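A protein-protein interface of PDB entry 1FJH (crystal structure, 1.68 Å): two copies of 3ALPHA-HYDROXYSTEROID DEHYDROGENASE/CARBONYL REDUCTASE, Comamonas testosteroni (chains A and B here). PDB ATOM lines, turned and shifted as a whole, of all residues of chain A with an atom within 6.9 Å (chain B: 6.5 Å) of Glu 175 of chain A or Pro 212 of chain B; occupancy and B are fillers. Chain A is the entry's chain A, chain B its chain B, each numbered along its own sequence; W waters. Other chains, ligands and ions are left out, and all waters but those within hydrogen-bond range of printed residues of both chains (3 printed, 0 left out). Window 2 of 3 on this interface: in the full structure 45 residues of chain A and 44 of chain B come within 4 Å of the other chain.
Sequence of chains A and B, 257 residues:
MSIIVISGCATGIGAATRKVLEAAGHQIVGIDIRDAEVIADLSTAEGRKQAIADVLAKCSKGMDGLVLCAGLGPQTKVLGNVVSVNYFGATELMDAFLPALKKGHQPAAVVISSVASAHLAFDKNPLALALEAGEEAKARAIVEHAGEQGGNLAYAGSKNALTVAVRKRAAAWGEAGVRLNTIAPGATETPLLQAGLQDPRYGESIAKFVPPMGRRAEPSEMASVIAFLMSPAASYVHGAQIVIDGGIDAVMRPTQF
Water W2 bridges O of Met 213 of chain B (2.8 Å) and O of Gly 174 of chain A (3.4 Å). Water W1 lies within hydrogen-bond range of OD1 of Asp 245 of chain B, O of His 238 of chain A and N of Ala 250 of chain B. Water W3 bridges OD1 of Asp 245 of chain B (3.0 Å) and N of His 238 of chain A (3.0 Å).
Printed residues of chain A that touch a printed residue of chain B: Ala 170, Ala 171, Gly 174, Glu 175 and His 238. Hydrophobic or aromatic side chains of chain B that line the printed part of chain A: Pro 212, Met 213 and Ala 250. Along chain B the printed residues that touch a printed residue of chain A span positions 212 to 250. Among the printed residues, no Asp or Glu carboxylate lies within 4 Å of a Lys or Arg side-chain nitrogen of the other chain.
Ala 170 of chain A touches Pro 212 of chain B. CB of Ala 170 of chain A touches CB of Ala 250 of chain B, 3.6 Å away. CA of Ala 171 of chain A touches CB of Pro 212 of chain B, at 3.99 Å. Gly 174 of chain A touches Met 213 of chain B (CA to SD, 3.8 Å). Pro 212 of chain B touches His 238 of chain A. CG of His 238 of chain A touches SD of Met 213 of chain B, 3.7 Å away. His 238 of chain A touches Asp 245 of chain B (O to OD1, 3.96 Å). His 238 of chain A touches Gly 246 of chain B.
Of the printed residues of chain B, Ala 170 of chain A touches Pro 212 and Ala 250. Of chain B, only Pro 212 comes within 4 Å of Glu 175 of chain A. Of the printed residues of chain A, Pro 212 of chain B touches Ala 170, Ala 171, Gly 174, Glu 175 and His 238. Of the printed residues of chain A, Met 213 of chain B touches Gly 174 (3.8 Å) and His 238 (3.7 Å). Of the printed residues of chain A, Asp 245 of chain B touches His 238 (3.96 Å). Of the printed residues of chain A, Gly 246 of chain B touches His 238. Of the printed residues of chain A, Ala 250 of chain B touches Ala 170. The nearest printed residue of chain B that does not touch His 238 of chain A is Ala 250 of chain B (4.8 Å).
O of Pro 212 of chain B is in hydrogen-bond range of N of Glu 175 of chain A. The backbone carbonyl oxygen (O) of His 238 of chain A sits close to the backbone NH (N) of Gly 247 of chain B (3.3 Å). O of Gly 174 of chain A sits close to O of Pro 212 of chain B, 3.1 Å away.
No position is printed for both chains. Of the 11 pairs that touch across the chains among the printed residues, none has its exchanged pair printed and touching as well.
The backbone carbonyl oxygen of Ala 170 of chain A is in hydrogen-bond range of a ring nitrogen (NE2) of His 238 of chain A. O of Gly 246 of chain B is in hydrogen-bond range of N of Met 213 of chain B (3.2 Å). N of Gly 247 of chain B sits at hydrogen-bond distance from OD1 of Asp 245 of chain B (2.9 Å). The side-chain carboxylate of Asp 245 of chain B is in hydrogen-bond range of the backbone NH of Asp 249 of chain B (2.7 Å).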
ATOM      1  N   LYS A 102     -13.123 -11.428   2.498  1.00  0.00           N
ATOM      2  CA  LYS A 102     -11.941 -11.581   3.341  1.00  0.00           C
ATOM      3  C   LYS A 102     -12.161 -10.964   4.727  1.00  0.00           C
ATOM      4  O   LYS A 102     -11.611 -11.438   5.724  1.00  0.00           O
ATOM      5  CB  LYS A 102     -10.750 -10.925   2.636  1.00  0.00           C
ATOM      6  CG  LYS A 102      -9.375 -11.363   3.099  1.00  0.00           C
ATOM      7  CD  LYS A 102      -8.332 -10.909   2.079  1.00  0.00           C
ATOM      8  CE  LYS A 102      -6.929 -11.357   2.445  1.00  0.00           C
ATOM      9  NZ  LYS A 102      -6.447 -10.702   3.688  1.00  0.00           N
ATOM     10  N   ARG A 169      -8.973 -20.647  -8.706  1.00  0.00           N
ATOM     11  CA  ARG A 169      -8.949 -19.596  -7.692  1.00  0.00           C
ATOM     12  C   ARG A 169      -8.847 -20.175  -6.281  1.00  0.00           C
ATOM     13  O   ARG A 169      -8.769 -19.431  -5.305  1.00  0.00           O
ATOM     14  CB  ARG A 169     -10.211 -18.735  -7.798  1.00  0.00           C
ATOM     15  CG  ARG A 169     -10.219 -17.798  -8.995  1.00  0.00           C
ATOM     16  CD  ARG A 169     -11.595 -17.180  -9.210  1.00  0.00           C
ATOM     17  NE  ARG A 169     -11.569 -16.124 -10.218  1.00  0.00           N
ATOM     18  CZ  ARG A 169     -11.252 -16.304 -11.500  1.00  0.00           C
ATOM     19  NH1 ARG A 169     -10.928 -17.508 -11.950  1.00  0.00           N
ATOM     20  NH2 ARG A 169     -11.261 -15.267 -12.334  1.00  0.00           N
ATOM     21  N   ALA A 170      -8.852 -21.501  -6.181  1.00  0.00           N
ATOM     22  CA  ALA A 170      -8.778 -22.182  -4.888  1.00  0.00           C
ATOM     23  C   ALA A 170      -7.581 -21.764  -4.042  1.00  0.00           C
ATOM     24  O   ALA A 170      -7.713 -21.517  -2.846  1.00  0.00           O
ATOM     25  CB  ALA A 170      -8.751 -23.687  -5.094  1.00  0.00           C
ATOM     26  N   ALA A 171      -6.407 -21.694  -4.659  1.00  0.00           N
ATOM     27  CA  ALA A 171      -5.204 -21.321  -3.924  1.00  0.00           C
ATOM     28  C   ALA A 171      -5.297 -19.911  -3.353  1.00  0.00           C
ATOM     29  O   ALA A 171      -5.094 -19.695  -2.157  1.00  0.00           O
ATOM     30  CB  ALA A 171      -3.985 -21.448  -4.829  1.00  0.00           C
ATOM     31  N   ALA A 172      -5.608 -18.949  -4.213  1.00  0.00           N
ATOM     32  CA  ALA A 172      -5.715 -17.564  -3.797  1.00  0.00           C
ATOM     33  C   ALA A 172      -6.816 -17.348  -2.764  1.00  0.00           C
ATOM     34  O   ALA A 172      -6.619 -16.630  -1.785  1.00  0.00           O
ATOM     35  CB  ALA A 172      -5.956 -16.677  -5.020  1.00  0.00           C
ATOM     36  N   TRP A 173      -7.977 -17.964  -2.977  1.00  0.00           N
ATOM     37  CA  TRP A 173      -9.083 -17.802  -2.038  1.00  0.00           C
ATOM     38  C   TRP A 173      -8.780 -18.486  -0.709  1.00  0.00           C
ATOM     39  O   TRP A 173      -9.158 -17.987   0.347  1.00  0.00           O
ATOM     40  CB  TRP A 173     -10.393 -18.335  -2.643  1.00  0.00           C
ATOM     41  CG  TRP A 173     -11.031 -17.350  -3.592  1.00  0.00           C
ATOM     42  CD1 TRP A 173     -10.452 -16.781  -4.692  1.00  0.00           C
ATOM     43  CD2 TRP A 173     -12.344 -16.776  -3.489  1.00  0.00           C
ATOM     44  NE1 TRP A 173     -11.319 -15.884  -5.277  1.00  0.00           N
ATOM     45  CE2 TRP A 173     -12.485 -15.861  -4.558  1.00  0.00           C
ATOM     46  CE3 TRP A 173     -13.413 -16.943  -2.595  1.00  0.00           C
ATOM     47  CZ2 TRP A 173     -13.656 -15.112  -4.756  1.00  0.00           C
ATOM     48  CZ3 TRP A 173     -14.580 -16.198  -2.793  1.00  0.00           C
ATOM     49  CH2 TRP A 173     -14.687 -15.294  -3.866  1.00  0.00           C
ATOM     50  N   GLY A 174      -8.095 -19.624  -0.769  1.00  0.00           N
ATOM     51  CA  GLY A 174      -7.735 -20.335   0.447  1.00  0.00           C
ATOM     52  C   GLY A 174      -6.754 -19.505   1.253  1.00  0.00           C
ATOM     53  O   GLY A 174      -6.866 -19.395   2.471  1.00  0.00           O
ATOM     54  N   GLU A 175      -5.785 -18.912   0.566  1.00  0.00           N
ATOM     55  CA  GLU A 175      -4.794 -18.069   1.226  1.00  0.00           C
ATOM     56  C   GLU A 175      -5.501 -16.891   1.893  1.00  0.00           C
ATOM     57  O   GLU A 175      -5.057 -16.403   2.928  1.00  0.00           O
ATOM     58  CB  GLU A 175      -3.773 -17.553   0.208  1.00  0.00           C
ATOM     59  CG  GLU A 175      -2.880 -18.630  -0.378  1.00  0.00           C
ATOM     60  CD  GLU A 175      -1.971 -18.096  -1.468  1.00  0.00           C
ATOM     61  OE1 GLU A 175      -1.265 -17.097  -1.218  1.00  0.00           O
ATOM     62  OE2 GLU A 175      -1.958 -18.679  -2.573  1.00  0.00           O
ATOM     63  N   ALA A 176      -6.603 -16.443   1.292  1.00  0.00           N
ATOM     64  CA  ALA A 176      -7.381 -15.329   1.826  1.00  0.00           C
ATOM     65  C   ALA A 176      -8.325 -15.773   2.941  1.00  0.00           C
ATOM     66  O   ALA A 176      -8.959 -14.943   3.590  1.00  0.00           O
ATOM     67  CB  ALA A 176      -8.185 -14.659   0.704  1.00  0.00           C
ATOM     68  N   GLY A 177      -8.428 -17.083   3.150  1.00  0.00           N
ATOM     69  CA  GLY A 177      -9.294 -17.604   4.196  1.00  0.00           C
ATOM     70  C   GLY A 177     -10.768 -17.666   3.828  1.00  0.00           C
ATOM     71  O   GLY A 177     -11.627 -17.710   4.711  1.00  0.00           O
ATOM     72  N   VAL A 178     -11.067 -17.679   2.532  1.00  0.00           N
ATOM     73  CA  VAL A 178     -12.457 -17.731   2.067  1.00  0.00           C
ATOM     74  C   VAL A 178     -12.713 -18.998   1.250  1.00  0.00           C
ATOM     75  O   VAL A 178     -12.042 -19.239   0.245  1.00  0.00           O
ATOM     76  CB  VAL A 178     -12.795 -16.501   1.184  1.00  0.00           C
ATOM     77  CG1 VAL A 178     -14.281 -16.501   0.823  1.00  0.00           C
ATOM     78  CG2 VAL A 178     -12.427 -15.211   1.914  1.00  0.00           C
ATOM     79  N   HIS A 238     -13.445 -27.155   0.096  1.00  0.00           N
ATOM     80  CA  HIS A 238     -12.984 -25.997  -0.653  1.00  0.00           C
ATOM     81  C   HIS A 238     -12.529 -26.395  -2.049  1.00  0.00           C
ATOM     82  O   HIS A 238     -11.835 -27.398  -2.221  1.00  0.00           O
ATOM     83  CB  HIS A 238     -11.820 -25.340   0.096  1.00  0.00           C
ATOM     84  CG  HIS A 238     -11.248 -24.149  -0.600  1.00  0.00           C
ATOM     85  ND1 HIS A 238     -12.012 -23.065  -0.972  1.00  0.00           N
ATOM     86  CD2 HIS A 238      -9.979 -23.863  -0.977  1.00  0.00           C
ATOM     87  CE1 HIS A 238     -11.239 -22.162  -1.549  1.00  0.00           C
ATOM     88  NE2 HIS A 238     -10.000 -22.623  -1.564  1.00  0.00           N
ATOM     89  N   VAL B 210       0.734 -28.420   2.108  1.00  0.00           N
ATOM     90  CA  VAL B 210      -0.174 -27.517   2.808  1.00  0.00           C
ATOM     91  C   VAL B 210      -1.357 -27.113   1.929  1.00  0.00           C
ATOM     92  O   VAL B 210      -1.188 -26.448   0.908  1.00  0.00           O
ATOM     93  CB  VAL B 210       0.565 -26.247   3.268  1.00  0.00           C
ATOM     94  CG1 VAL B 210      -0.365 -25.368   4.084  1.00  0.00           C
ATOM     95  CG2 VAL B 210       1.791 -26.633   4.087  1.00  0.00           C
ATOM     96  N   PRO B 211      -2.576 -27.514   2.318  1.00  0.00           N
ATOM     97  CA  PRO B 211      -3.778 -27.183   1.547  1.00  0.00           C
ATOM     98  C   PRO B 211      -4.020 -25.680   1.464  1.00  0.00           C
ATOM     99  O   PRO B 211      -3.555 -24.919   2.309  1.00  0.00           O
ATOM    100  CB  PRO B 211      -4.894 -27.890   2.319  1.00  0.00           C
ATOM    101  CG  PRO B 211      -4.181 -29.029   3.002  1.00  0.00           C
ATOM    102  CD  PRO B 211      -2.912 -28.369   3.469  1.00  0.00           C
ATOM    103  N   PRO B 212      -4.746 -25.234   0.429  1.00  0.00           N
ATOM    104  CA  PRO B 212      -5.040 -23.810   0.268  1.00  0.00           C
ATOM    105  C   PRO B 212      -5.649 -23.211   1.535  1.00  0.00           C
ATOM    106  O   PRO B 212      -5.344 -22.077   1.898  1.00  0.00           O
ATOM    107  CB  PRO B 212      -6.011 -23.801  -0.909  1.00  0.00           C
ATOM    108  CG  PRO B 212      -5.483 -24.902  -1.761  1.00  0.00           C
ATOM    109  CD  PRO B 212      -5.191 -25.998  -0.752  1.00  0.00           C
ATOM    110  N   MET B 213      -6.501 -23.975   2.217  1.00  0.00           N
ATOM    111  CA  MET B 213      -7.123 -23.476   3.437  1.00  0.00           C
ATOM    112  C   MET B 213      -6.128 -23.357   4.599  1.00  0.00           C
ATOM    113  O   MET B 213      -6.484 -22.885   5.674  1.00  0.00           O
ATOM    114  CB  MET B 213      -8.318 -24.348   3.842  1.00  0.00           C
ATOM    115  CG  MET B 213      -9.531 -24.250   2.900  1.00  0.00           C
ATOM    116  SD  MET B 213     -10.099 -22.553   2.487  1.00  0.00           S
ATOM    117  CE  MET B 213     -10.614 -21.926   4.093  1.00  0.00           C
ATOM    118  N   GLY B 214      -4.896 -23.811   4.374  1.00  0.00           N
ATOM    119  CA  GLY B 214      -3.836 -23.686   5.367  1.00  0.00           C
ATOM    120  C   GLY B 214      -3.771 -24.528   6.630  1.00  0.00           C
ATOM    121  O   GLY B 214      -3.182 -24.089   7.623  1.00  0.00           O
ATOM    122  N   ARG B 215      -4.342 -25.727   6.615  1.00  0.00           N
ATOM    123  CA  ARG B 215      -4.300 -26.573   7.803  1.00  0.00           C
ATOM    124  C   ARG B 215      -4.785 -27.984   7.522  1.00  0.00           C
ATOM    125  O   ARG B 215      -5.350 -28.258   6.467  1.00  0.00           O
ATOM    126  CB  ARG B 215      -5.158 -25.965   8.909  1.00  0.00           C
ATOM    127  CG  ARG B 215      -6.634 -25.908   8.567  1.00  0.00           C
ATOM    128  CD  ARG B 215      -7.432 -25.205   9.651  1.00  0.00           C
ATOM    129  NE  ARG B 215      -8.850 -25.138   9.312  1.00  0.00           N
ATOM    130  CZ  ARG B 215      -9.649 -26.196   9.226  1.00  0.00           C
ATOM    131  NH1 ARG B 215      -9.174 -27.413   9.460  1.00  0.00           N
ATOM    132  NH2 ARG B 215     -10.923 -26.038   8.891  1.00  0.00           N
ATOM    133  N   ASP B 245     -10.906 -31.779   1.172  1.00  0.00           N
ATOM    134  CA  ASP B 245      -9.452 -31.713   1.256  1.00  0.00           C
ATOM    135  C   ASP B 245      -8.835 -30.321   1.368  1.00  0.00           C
ATOM    136  O   ASP B 245      -7.642 -30.148   1.110  1.00  0.00           O
ATOM    137  CB  ASP B 245      -8.852 -32.428   0.041  1.00  0.00           C
ATOM    138  CG  ASP B 245      -9.064 -31.661  -1.262  1.00  0.00           C
ATOM    139  OD1 ASP B 245      -9.793 -30.648  -1.263  1.00  0.00           O
ATOM    140  OD2 ASP B 245      -8.492 -32.083  -2.292  1.00  0.00           O
ATOM    141  N   GLY B 246      -9.640 -29.333   1.734  1.00  0.00           N
ATOM    142  CA  GLY B 246      -9.112 -27.990   1.885  1.00  0.00           C
ATOM    143  C   GLY B 246      -8.662 -27.325   0.596  1.00  0.00           C
ATOM    144  O   GLY B 246      -8.005 -26.285   0.649  1.00  0.00           O
ATOM    145  N   GLY B 247      -8.982 -27.925  -0.549  1.00  0.00           N
ATOM    146  CA  GLY B 247      -8.627 -27.318  -1.824  1.00  0.00           C
ATOM    147  C   GLY B 247      -7.505 -27.926  -2.642  1.00  0.00           C
ATOM    148  O   GLY B 247      -7.270 -27.502  -3.776  1.00  0.00           O
ATOM    149  N   ILE B 248      -6.821 -28.921  -2.093  1.00  0.00           N
ATOM    150  CA  ILE B 248      -5.707 -29.552  -2.799  1.00  0.00           C
ATOM    151  C   ILE B 248      -6.054 -30.062  -4.193  1.00  0.00           C
ATOM    152  O   ILE B 248      -5.348 -29.768  -5.164  1.00  0.00           O
ATOM    153  CB  ILE B 248      -5.128 -30.728  -1.975  1.00  0.00           C
ATOM    154  CG1 ILE B 248      -4.462 -30.192  -0.709  1.00  0.00           C
ATOM    155  CG2 ILE B 248      -4.120 -31.514  -2.813  1.00  0.00           C
ATOM    156  CD1 ILE B 248      -3.244 -29.335  -0.974  1.00  0.00           C
ATOM    157  N   ASP B 249      -7.133 -30.831  -4.293  1.00  0.00           N
ATOM    158  CA  ASP B 249      -7.552 -31.392  -5.571  1.00  0.00           C
ATOM    159  C   ASP B 249      -7.799 -30.308  -6.622  1.00  0.00           C
ATOM    160  O   ASP B 249      -7.443 -30.468  -7.795  1.00  0.00           O
ATOM    161  CB  ASP B 249      -8.813 -32.234  -5.371  1.00  0.00           C
ATOM    162  CG  ASP B 249      -9.259 -32.925  -6.637  1.00  0.00           C
ATOM    163  OD1 ASP B 249      -8.498 -33.773  -7.149  1.00  0.00           O
ATOM    164  OD2 ASP B 249     -10.367 -32.618  -7.121  1.00  0.00           O
ATOM    165  N   ALA B 250      -8.398 -29.198  -6.200  1.00  0.00           N
ATOM    166  CA  ALA B 250      -8.672 -28.095  -7.113  1.00  0.00           C
ATOM    167  C   ALA B 250      -7.369 -27.515  -7.663  1.00  0.00           C
ATOM    168  O   ALA B 250      -7.286 -27.163  -8.838  1.00  0.00           O
ATOM    169  CB  ALA B 250      -9.469 -27.010  -6.398  1.00  0.00           C
ATOM    170  N   VAL B 251      -6.351 -27.424  -6.810  1.00  0.00           N
ATOM    171  CA  VAL B 251      -5.059 -26.880  -7.222  1.00  0.00           C
ATOM    172  C   VAL B 251      -4.307 -27.838  -8.146  1.00  0.00           C
ATOM    173  O   VAL B 251      -3.714 -27.415  -9.142  1.00  0.00           O
ATOM    174  CB  VAL B 251      -4.166 -26.560  -5.991  1.00  0.00           C
ATOM    175  CG1 VAL B 251      -2.765 -26.162  -6.448  1.00  0.00           C
ATOM    176  CG2 VAL B 251      -4.777 -25.429  -5.183  1.00  0.00           C
HETATM  177  O   HOH W   1     -10.785 -29.627  -3.707  1.00  0.00           O
HETATM  178  O   HOH W   2      -7.808 -20.451   5.519  1.00  0.00           O
HETATM  179  O   HOH W   3     -12.566 -29.933  -0.542  1.00  0.00           O
